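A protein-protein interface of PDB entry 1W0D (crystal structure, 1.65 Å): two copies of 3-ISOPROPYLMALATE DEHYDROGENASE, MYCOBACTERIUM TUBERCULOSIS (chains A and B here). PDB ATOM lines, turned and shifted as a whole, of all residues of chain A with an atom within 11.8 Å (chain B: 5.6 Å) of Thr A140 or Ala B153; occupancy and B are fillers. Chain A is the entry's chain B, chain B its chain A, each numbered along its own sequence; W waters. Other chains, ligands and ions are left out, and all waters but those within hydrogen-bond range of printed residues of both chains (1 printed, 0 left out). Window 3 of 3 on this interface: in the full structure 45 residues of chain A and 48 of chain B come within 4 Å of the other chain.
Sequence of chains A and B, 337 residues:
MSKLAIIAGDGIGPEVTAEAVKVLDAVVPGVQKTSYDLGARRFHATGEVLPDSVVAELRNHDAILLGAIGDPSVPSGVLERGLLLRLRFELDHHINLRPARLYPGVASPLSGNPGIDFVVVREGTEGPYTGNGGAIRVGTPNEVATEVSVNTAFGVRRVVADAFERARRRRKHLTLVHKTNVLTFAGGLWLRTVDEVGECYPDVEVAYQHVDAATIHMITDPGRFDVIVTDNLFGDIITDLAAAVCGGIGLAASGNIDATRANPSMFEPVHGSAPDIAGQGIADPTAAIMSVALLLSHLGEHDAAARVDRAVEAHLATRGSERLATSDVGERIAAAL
O of Glu A143 lies within hydrogen-bond range of N of Ala B153 (2.9 Å).
The backbone NH (N) of Ala A145 is in hydrogen-bond range of the backbone carbonyl oxygen (O) of Asn B151 (2.7 Å).
OG1 of Thr A140 is in hydrogen-bond range of O of Arg A137, 2.6 Å away.
The side-chain hydroxyl of Thr A140 sits at hydrogen-bond distance from the backbone NH of Glu A143 (3.3 Å).
The backbone NH (N) of Ile A136 sits at hydrogen-bond distance from the backbone carbonyl oxygen (O) of Val A144 (2.9 Å).
The side-chain hydroxyl of Thr A140 lies close to the backbone NH of Asn A142, at 3.0 Å.
N of Glu A143 sits close to O of Arg A137, at 3.5 Å.
The backbone NH (N) of Gly B155 lies within hydrogen-bond range of the side-chain hydroxyl (OG1) of Thr B152 (2.8 Å).
Ala B153 touches Thr A140.
Pro A141 touches Ala B153.
O of Pro A141 touches N of Phe B154 (3.8 Å).
Glu A143 touches Thr B152.
CD of Glu A143 touches CD1 of Leu B189 (3.6 Å).
Val A144 touches Asn B151.
Printed residues of chain B within 4 Å of Pro A141: Ala B153 and Phe B154.
Of the printed residues of chain B, Val A144 touches Asn B151.
Of the printed residues of chain B, Ala A145 touches Asn B151 (2.7 Å).
Thr A146 touches none of the printed residues of chain B.
Of the printed residues of chain A, Asn B151 touches Val A144 and Ala A145.
Thr B152 touches just one residue of chain A: Glu A143.
Ala B153 touches just these residues of chain A: Thr A140 (3.3 Å), Pro A141 (3.5 Å) and Glu A143 (2.9 Å).
Phe B154 touches one residue of chain A.
Of the printed residues of chain A, Leu B189 touches Glu A143 (3.6 Å).
The nearest printed residue of chain A that does not touch Leu B189 is Ala A145 (4.2 Å).
Of the 11 printed residues of chain B, 5 touch a printed residue of chain A.
Printed residues of chain B that touch a printed residue of chain A: Asn B151, Thr B152, Ala B153, Phe B154 and Leu B189.
Hydrophobic or aromatic side chains of chain A within 4 Å of the printed part of chain B: Val A144.
Among the printed residues, 8 pairs touch across the chains.
No position is printed for both chains.
Of the 8 pairs that touch across the chains among the printed residues, none has its exchanged pair printed and touching as well.
Water W1 lies within hydrogen-bond range of the backbone carbonyl oxygen (O) of Pro A141 (2.8 Å), the backbone carbonyl oxygen (O) of Glu A143 (2.8 Å), the backbone NH (N) of Phe B154 (3.0 Å) and the backbone NH (N) of Ala B153 (3.2 Å).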
ATOM      1  N   GLY A 134      18.866  28.540  18.657  1.00  0.00           N
ATOM      2  CA  GLY A 134      19.836  29.505  18.249  1.00  0.00           C
ATOM      3  C   GLY A 134      21.101  28.743  17.976  1.00  0.00           C
ATOM      4  O   GLY A 134      21.108  27.523  17.973  1.00  0.00           O
ATOM      5  N   ALA A 135      22.170  29.473  17.761  1.00  0.00           N
ATOM      6  CA  ALA A 135      23.415  28.811  17.408  1.00  0.00           C
ATOM      7  C   ALA A 135      24.544  29.621  17.967  1.00  0.00           C
ATOM      8  O   ALA A 135      24.417  30.841  18.159  1.00  0.00           O
ATOM      9  CB  ALA A 135      23.571  28.674  15.900  1.00  0.00           C
ATOM     10  N   ILE A 136      25.658  28.955  18.190  1.00  0.00           N
ATOM     11  CA  ILE A 136      26.872  29.646  18.557  1.00  0.00           C
ATOM     12  C   ILE A 136      27.956  29.096  17.695  1.00  0.00           C
ATOM     13  O   ILE A 136      27.877  27.986  17.168  1.00  0.00           O
ATOM     14  CB  ILE A 136      27.182  29.444  20.065  1.00  0.00           C
ATOM     15  CG1 ILE A 136      27.220  27.953  20.376  1.00  0.00           C
ATOM     16  CG2 ILE A 136      26.105  30.083  20.960  1.00  0.00           C
ATOM     17  CD1 ILE A 136      27.906  27.598  21.667  1.00  0.00           C
ATOM     18  N   ARG A 137      28.948  29.948  17.489  1.00  0.00           N
ATOM     19  CA  ARG A 137      30.130  29.638  16.750  1.00  0.00           C
ATOM     20  C   ARG A 137      29.745  29.187  15.351  1.00  0.00           C
ATOM     21  O   ARG A 137      30.310  28.288  14.812  1.00  0.00           O
ATOM     22  CB  ARG A 137      30.932  28.565  17.492  1.00  0.00           C
ATOM     23  CG  ARG A 137      31.218  29.053  18.914  1.00  0.00           C
ATOM     24  CD  ARG A 137      32.405  28.373  19.599  1.00  0.00           C
ATOM     25  NE  ARG A 137      32.557  28.934  20.910  1.00  0.00           N
ATOM     26  CZ  ARG A 137      32.120  28.410  22.062  1.00  0.00           C
ATOM     27  NH1 ARG A 137      31.578  27.195  22.126  1.00  0.00           N
ATOM     28  NH2 ARG A 137      32.293  29.129  23.168  1.00  0.00           N
ATOM     29  N   VAL A 138      28.757  29.869  14.774  1.00  0.00           N
ATOM     30  CA  VAL A 138      28.342  29.492  13.407  1.00  0.00           C
ATOM     31  C   VAL A 138      29.435  29.507  12.394  1.00  0.00           C
ATOM     32  O   VAL A 138      30.309  30.403  12.393  1.00  0.00           O
ATOM     33  CB  VAL A 138      27.171  30.354  12.906  1.00  0.00           C
ATOM     34  CG1 VAL A 138      26.876  30.045  11.423  1.00  0.00           C
ATOM     35  CG2 VAL A 138      25.995  30.047  13.692  1.00  0.00           C
ATOM     36  N   GLY A 139      29.455  28.493  11.525  1.00  0.00           N
ATOM     37  CA  GLY A 139      30.321  28.514  10.359  1.00  0.00           C
ATOM     38  C   GLY A 139      31.695  28.039  10.734  1.00  0.00           C
ATOM     39  O   GLY A 139      32.638  28.130   9.963  1.00  0.00           O
ATOM     40  N   THR A 140      31.797  27.476  11.941  1.00  0.00           N
ATOM     41  CA  THR A 140      33.060  26.884  12.373  1.00  0.00           C
ATOM     42  C   THR A 140      32.825  25.421  12.754  1.00  0.00           C
ATOM     43  O   THR A 140      31.683  25.002  12.916  1.00  0.00           O
ATOM     44  CB  THR A 140      33.576  27.607  13.662  1.00  0.00           C
ATOM     45  OG1 THR A 140      32.743  27.245  14.757  1.00  0.00           O
ATOM     46  CG2 THR A 140      33.458  29.123  13.563  1.00  0.00           C
ATOM     47  N   PRO A 141      33.897  24.676  12.975  1.00  0.00           N
ATOM     48  CA  PRO A 141      33.743  23.289  13.424  1.00  0.00           C
ATOM     49  C   PRO A 141      33.223  23.252  14.835  1.00  0.00           C
ATOM     50  O   PRO A 141      32.881  22.151  15.292  1.00  0.00           O
ATOM     51  CB  PRO A 141      35.174  22.775  13.426  1.00  0.00           C
ATOM     52  CG  PRO A 141      35.889  23.718  12.398  1.00  0.00           C
ATOM     53  CD  PRO A 141      35.312  25.015  12.798  1.00  0.00           C
ATOM     54  N   ASN A 142      33.182  24.404  15.512  1.00  0.00           N
ATOM     55  CA  ASN A 142      32.592  24.433  16.837  1.00  0.00           C
ATOM     56  C   ASN A 142      31.133  24.852  16.870  1.00  0.00           C
ATOM     57  O   ASN A 142      30.580  25.104  17.922  1.00  0.00           O
ATOM     58  CB  ASN A 142      33.426  25.373  17.718  1.00  0.00           C
ATOM     59  CG  ASN A 142      34.900  25.168  17.463  1.00  0.00           C
ATOM     60  OD1 ASN A 142      35.621  26.015  16.893  1.00  0.00           O
ATOM     61  ND2 ASN A 142      35.349  23.986  17.824  1.00  0.00           N
ATOM     62  N   GLU A 143      30.515  24.948  15.701  1.00  0.00           N
ATOM     63  CA  GLU A 143      29.118  25.379  15.729  1.00  0.00           C
ATOM     64  C   GLU A 143      28.251  24.421  16.552  1.00  0.00           C
ATOM     65  O   GLU A 143      28.382  23.211  16.479  1.00  0.00           O
ATOM     66  CB  GLU A 143      28.587  25.476  14.307  1.00  0.00           C
ATOM     67  CG  GLU A 143      27.133  25.968  14.260  1.00  0.00           C
ATOM     68  CD  GLU A 143      26.751  26.339  12.807  1.00  0.00           C
ATOM     69  OE1 GLU A 143      27.641  26.345  11.976  1.00  0.00           O
ATOM     70  OE2 GLU A 143      25.498  26.519  12.596  1.00  0.00           O
ATOM     71  N   VAL A 144      27.377  25.004  17.303  1.00  0.00           N
ATOM     72  CA  VAL A 144      26.388  24.284  18.038  1.00  0.00           C
ATOM     73  C   VAL A 144      25.102  24.970  17.763  1.00  0.00           C
ATOM     74  O   VAL A 144      24.975  26.162  17.968  1.00  0.00           O
ATOM     75  CB  VAL A 144      26.679  24.217  19.564  1.00  0.00           C
ATOM     76  CG1 VAL A 144      25.554  23.386  20.223  1.00  0.00           C
ATOM     77  CG2 VAL A 144      28.025  23.541  19.805  1.00  0.00           C
ATOM     78  N   ALA A 145      24.122  24.188  17.349  1.00  0.00           N
ATOM     79  CA  ALA A 145      22.811  24.750  17.042  1.00  0.00           C
ATOM     80  C   ALA A 145      21.753  24.024  17.812  1.00  0.00           C
ATOM     81  O   ALA A 145      21.720  22.774  17.853  1.00  0.00           O
ATOM     82  CB  ALA A 145      22.531  24.640  15.503  1.00  0.00           C
ATOM     83  N   THR A 146      20.837  24.782  18.433  1.00  0.00           N
ATOM     84  CA  THR A 146      19.839  24.131  19.209  1.00  0.00           C
ATOM     85  C   THR A 146      18.466  24.441  18.637  1.00  0.00           C
ATOM     86  O   THR A 146      18.217  25.505  18.025  1.00  0.00           O
ATOM     87  CB  THR A 146      19.880  24.611  20.652  1.00  0.00           C
ATOM     88  OG1 THR A 146      19.646  26.027  20.646  1.00  0.00           O
ATOM     89  CG2 THR A 146      21.253  24.473  21.234  1.00  0.00           C
ATOM     90  N   GLU B 126      23.232  12.740  18.186  1.00  0.00           N
ATOM     91  CA  GLU B 126      22.749  14.033  18.703  1.00  0.00           C
ATOM     92  C   GLU B 126      21.321  14.295  18.300  1.00  0.00           C
ATOM     93  O   GLU B 126      20.570  13.357  18.087  1.00  0.00           O
ATOM     94  CB  GLU B 126      23.714  15.170  18.338  1.00  0.00           C
ATOM     95  CG  GLU B 126      23.894  15.345  16.835  1.00  0.00           C
ATOM     96  CD  GLU B 126      24.870  16.453  16.454  1.00  0.00           C
ATOM     97  OE1 GLU B 126      25.981  16.536  17.029  1.00  0.00           O
ATOM     98  OE2 GLU B 126      24.493  17.218  15.526  1.00  0.00           O
ATOM     99  N   ASN B 151      22.565  20.152  18.062  1.00  0.00           N
ATOM    100  CA  ASN B 151      23.145  19.772  16.799  1.00  0.00           C
ATOM    101  C   ASN B 151      24.494  20.416  16.732  1.00  0.00           C
ATOM    102  O   ASN B 151      24.678  21.532  17.201  1.00  0.00           O
ATOM    103  CB  ASN B 151      22.279  20.340  15.682  1.00  0.00           C
ATOM    104  CG  ASN B 151      20.858  19.837  15.808  1.00  0.00           C
ATOM    105  OD1 ASN B 151      20.553  18.782  15.257  1.00  0.00           O
ATOM    106  ND2 ASN B 151      20.016  20.501  16.638  1.00  0.00           N
ATOM    107  N   THR B 152      25.463  19.724  16.196  1.00  0.00           N
ATOM    108  CA  THR B 152      26.803  20.288  16.246  1.00  0.00           C
ATOM    109  C   THR B 152      27.494  20.074  14.914  1.00  0.00           C
ATOM    110  O   THR B 152      27.249  19.096  14.194  1.00  0.00           O
ATOM    111  CB  THR B 152      27.677  19.622  17.318  1.00  0.00           C
ATOM    112  OG1 THR B 152      27.873  18.232  16.986  1.00  0.00           O
ATOM    113  CG2 THR B 152      26.991  19.640  18.667  1.00  0.00           C
ATOM    114  N   ALA B 153      28.316  21.020  14.534  1.00  0.00           N
ATOM    115  CA  ALA B 153      29.151  20.883  13.353  1.00  0.00           C
ATOM    116  C   ALA B 153      29.984  19.602  13.423  1.00  0.00           C
ATOM    117  O   ALA B 153      30.109  18.855  12.453  1.00  0.00           O
ATOM    118  CB  ALA B 153      30.057  22.129  13.151  1.00  0.00           C
ATOM    119  N   PHE B 154      30.449  19.306  14.621  1.00  0.00           N
ATOM    120  CA  PHE B 154      31.200  18.090  14.849  1.00  0.00           C
ATOM    121  C   PHE B 154      30.374  16.874  14.401  1.00  0.00           C
ATOM    122  O   PHE B 154      30.859  16.085  13.561  1.00  0.00           O
ATOM    123  CB  PHE B 154      31.528  17.972  16.323  1.00  0.00           C
ATOM    124  CG  PHE B 154      32.235  16.720  16.679  1.00  0.00           C
ATOM    125  CD1 PHE B 154      33.535  16.480  16.275  1.00  0.00           C
ATOM    126  CD2 PHE B 154      31.566  15.762  17.427  1.00  0.00           C
ATOM    127  CE1 PHE B 154      34.188  15.304  16.627  1.00  0.00           C
ATOM    128  CE2 PHE B 154      32.226  14.600  17.805  1.00  0.00           C
ATOM    129  CZ  PHE B 154      33.508  14.370  17.397  1.00  0.00           C
ATOM    130  N   GLY B 155      29.190  16.722  14.971  1.00  0.00           N
ATOM    131  CA  GLY B 155      28.326  15.577  14.677  1.00  0.00           C
ATOM    132  C   GLY B 155      27.873  15.588  13.261  1.00  0.00           C
ATOM    133  O   GLY B 155      27.856  14.512  12.612  1.00  0.00           O
ATOM    134  N   VAL B 156      27.416  16.743  12.787  1.00  0.00           N
ATOM    135  CA  VAL B 156      26.849  16.784  11.466  1.00  0.00           C
ATOM    136  C   VAL B 156      27.882  16.540  10.373  1.00  0.00           C
ATOM    137  O   VAL B 156      27.618  15.789   9.396  1.00  0.00           O
ATOM    138  CB  VAL B 156      26.116  18.111  11.240  1.00  0.00           C
ATOM    139  CG1 VAL B 156      25.652  18.216   9.762  1.00  0.00           C
ATOM    140  CG2 VAL B 156      24.909  18.219  12.196  1.00  0.00           C
ATOM    141  N   ARG B 157      29.059  17.161  10.495  1.00  0.00           N
ATOM    142  CA  ARG B 157      30.004  17.023   9.418  1.00  0.00           C
ATOM    143  C   ARG B 157      30.410  15.544   9.224  1.00  0.00           C
ATOM    144  O   ARG B 157      30.611  15.099   8.101  1.00  0.00           O
ATOM    145  CB  ARG B 157      31.266  17.870   9.676  1.00  0.00           C
ATOM    146  CG  ARG B 157      32.039  17.987   8.418  1.00  0.00           C
ATOM    147  CD  ARG B 157      33.401  18.652   8.568  1.00  0.00           C
ATOM    148  NE  ARG B 157      34.039  18.742   7.245  1.00  0.00           N
ATOM    149  CZ  ARG B 157      34.613  17.720   6.610  1.00  0.00           C
ATOM    150  NH1 ARG B 157      34.671  16.515   7.163  1.00  0.00           N
ATOM    151  NH2 ARG B 157      35.153  17.911   5.402  1.00  0.00           N
ATOM    152  N   ARG B 158      30.552  14.821  10.326  1.00  0.00           N
ATOM    153  CA  ARG B 158      30.991  13.431  10.262  1.00  0.00           C
ATOM    154  C   ARG B 158      30.018  12.613   9.457  1.00  0.00           C
ATOM    155  O   ARG B 158      30.386  11.749   8.665  1.00  0.00           O
ATOM    156  CB  ARG B 158      30.878  12.839  11.661  1.00  0.00           C
ATOM    157  CG  ARG B 158      31.781  13.386  12.676  1.00  0.00           C
ATOM    158  CD  ARG B 158      31.873  12.470  13.848  1.00  0.00           C
ATOM    159  NE  ARG B 158      30.698  12.464  14.687  1.00  0.00           N
ATOM    160  CZ  ARG B 158      30.724  12.000  15.915  1.00  0.00           C
ATOM    161  NH1 ARG B 158      31.876  11.536  16.396  1.00  0.00           N
ATOM    162  NH2 ARG B 158      29.648  12.020  16.669  1.00  0.00           N
ATOM    163  N   LEU B 189      22.639  24.617   9.912  1.00  0.00           N
ATOM    164  CA  LEU B 189      23.867  23.884  10.111  1.00  0.00           C
ATOM    165  C   LEU B 189      23.957  22.729   9.140  1.00  0.00           C
ATOM    166  O   LEU B 189      25.038  22.492   8.579  1.00  0.00           O
ATOM    167  CB  LEU B 189      23.968  23.356  11.545  1.00  0.00           C
ATOM    168  CG  LEU B 189      25.115  22.389  11.890  1.00  0.00           C
ATOM    169  CD1 LEU B 189      26.488  22.940  11.686  1.00  0.00           C
ATOM    170  CD2 LEU B 189      24.947  21.949  13.320  1.00  0.00           C
ATOM    171  N   THR B 193      26.645  22.572   6.141  1.00  0.00           N
ATOM    172  CA  THR B 193      27.649  21.525   6.244  1.00  0.00           C
ATOM    173  C   THR B 193      27.621  20.660   4.977  1.00  0.00           C
ATOM    174  O   THR B 193      28.683  20.291   4.435  1.00  0.00           O
ATOM    175  CB  THR B 193      27.346  20.643   7.469  1.00  0.00           C
ATOM    176  OG1 THR B 193      27.477  21.445   8.666  1.00  0.00           O
ATOM    177  CG2 THR B 193      28.422  19.567   7.599  1.00  0.00           C
HETATM  178  O   HOH W   1      30.607  21.452  16.707  1.00  0.00           O
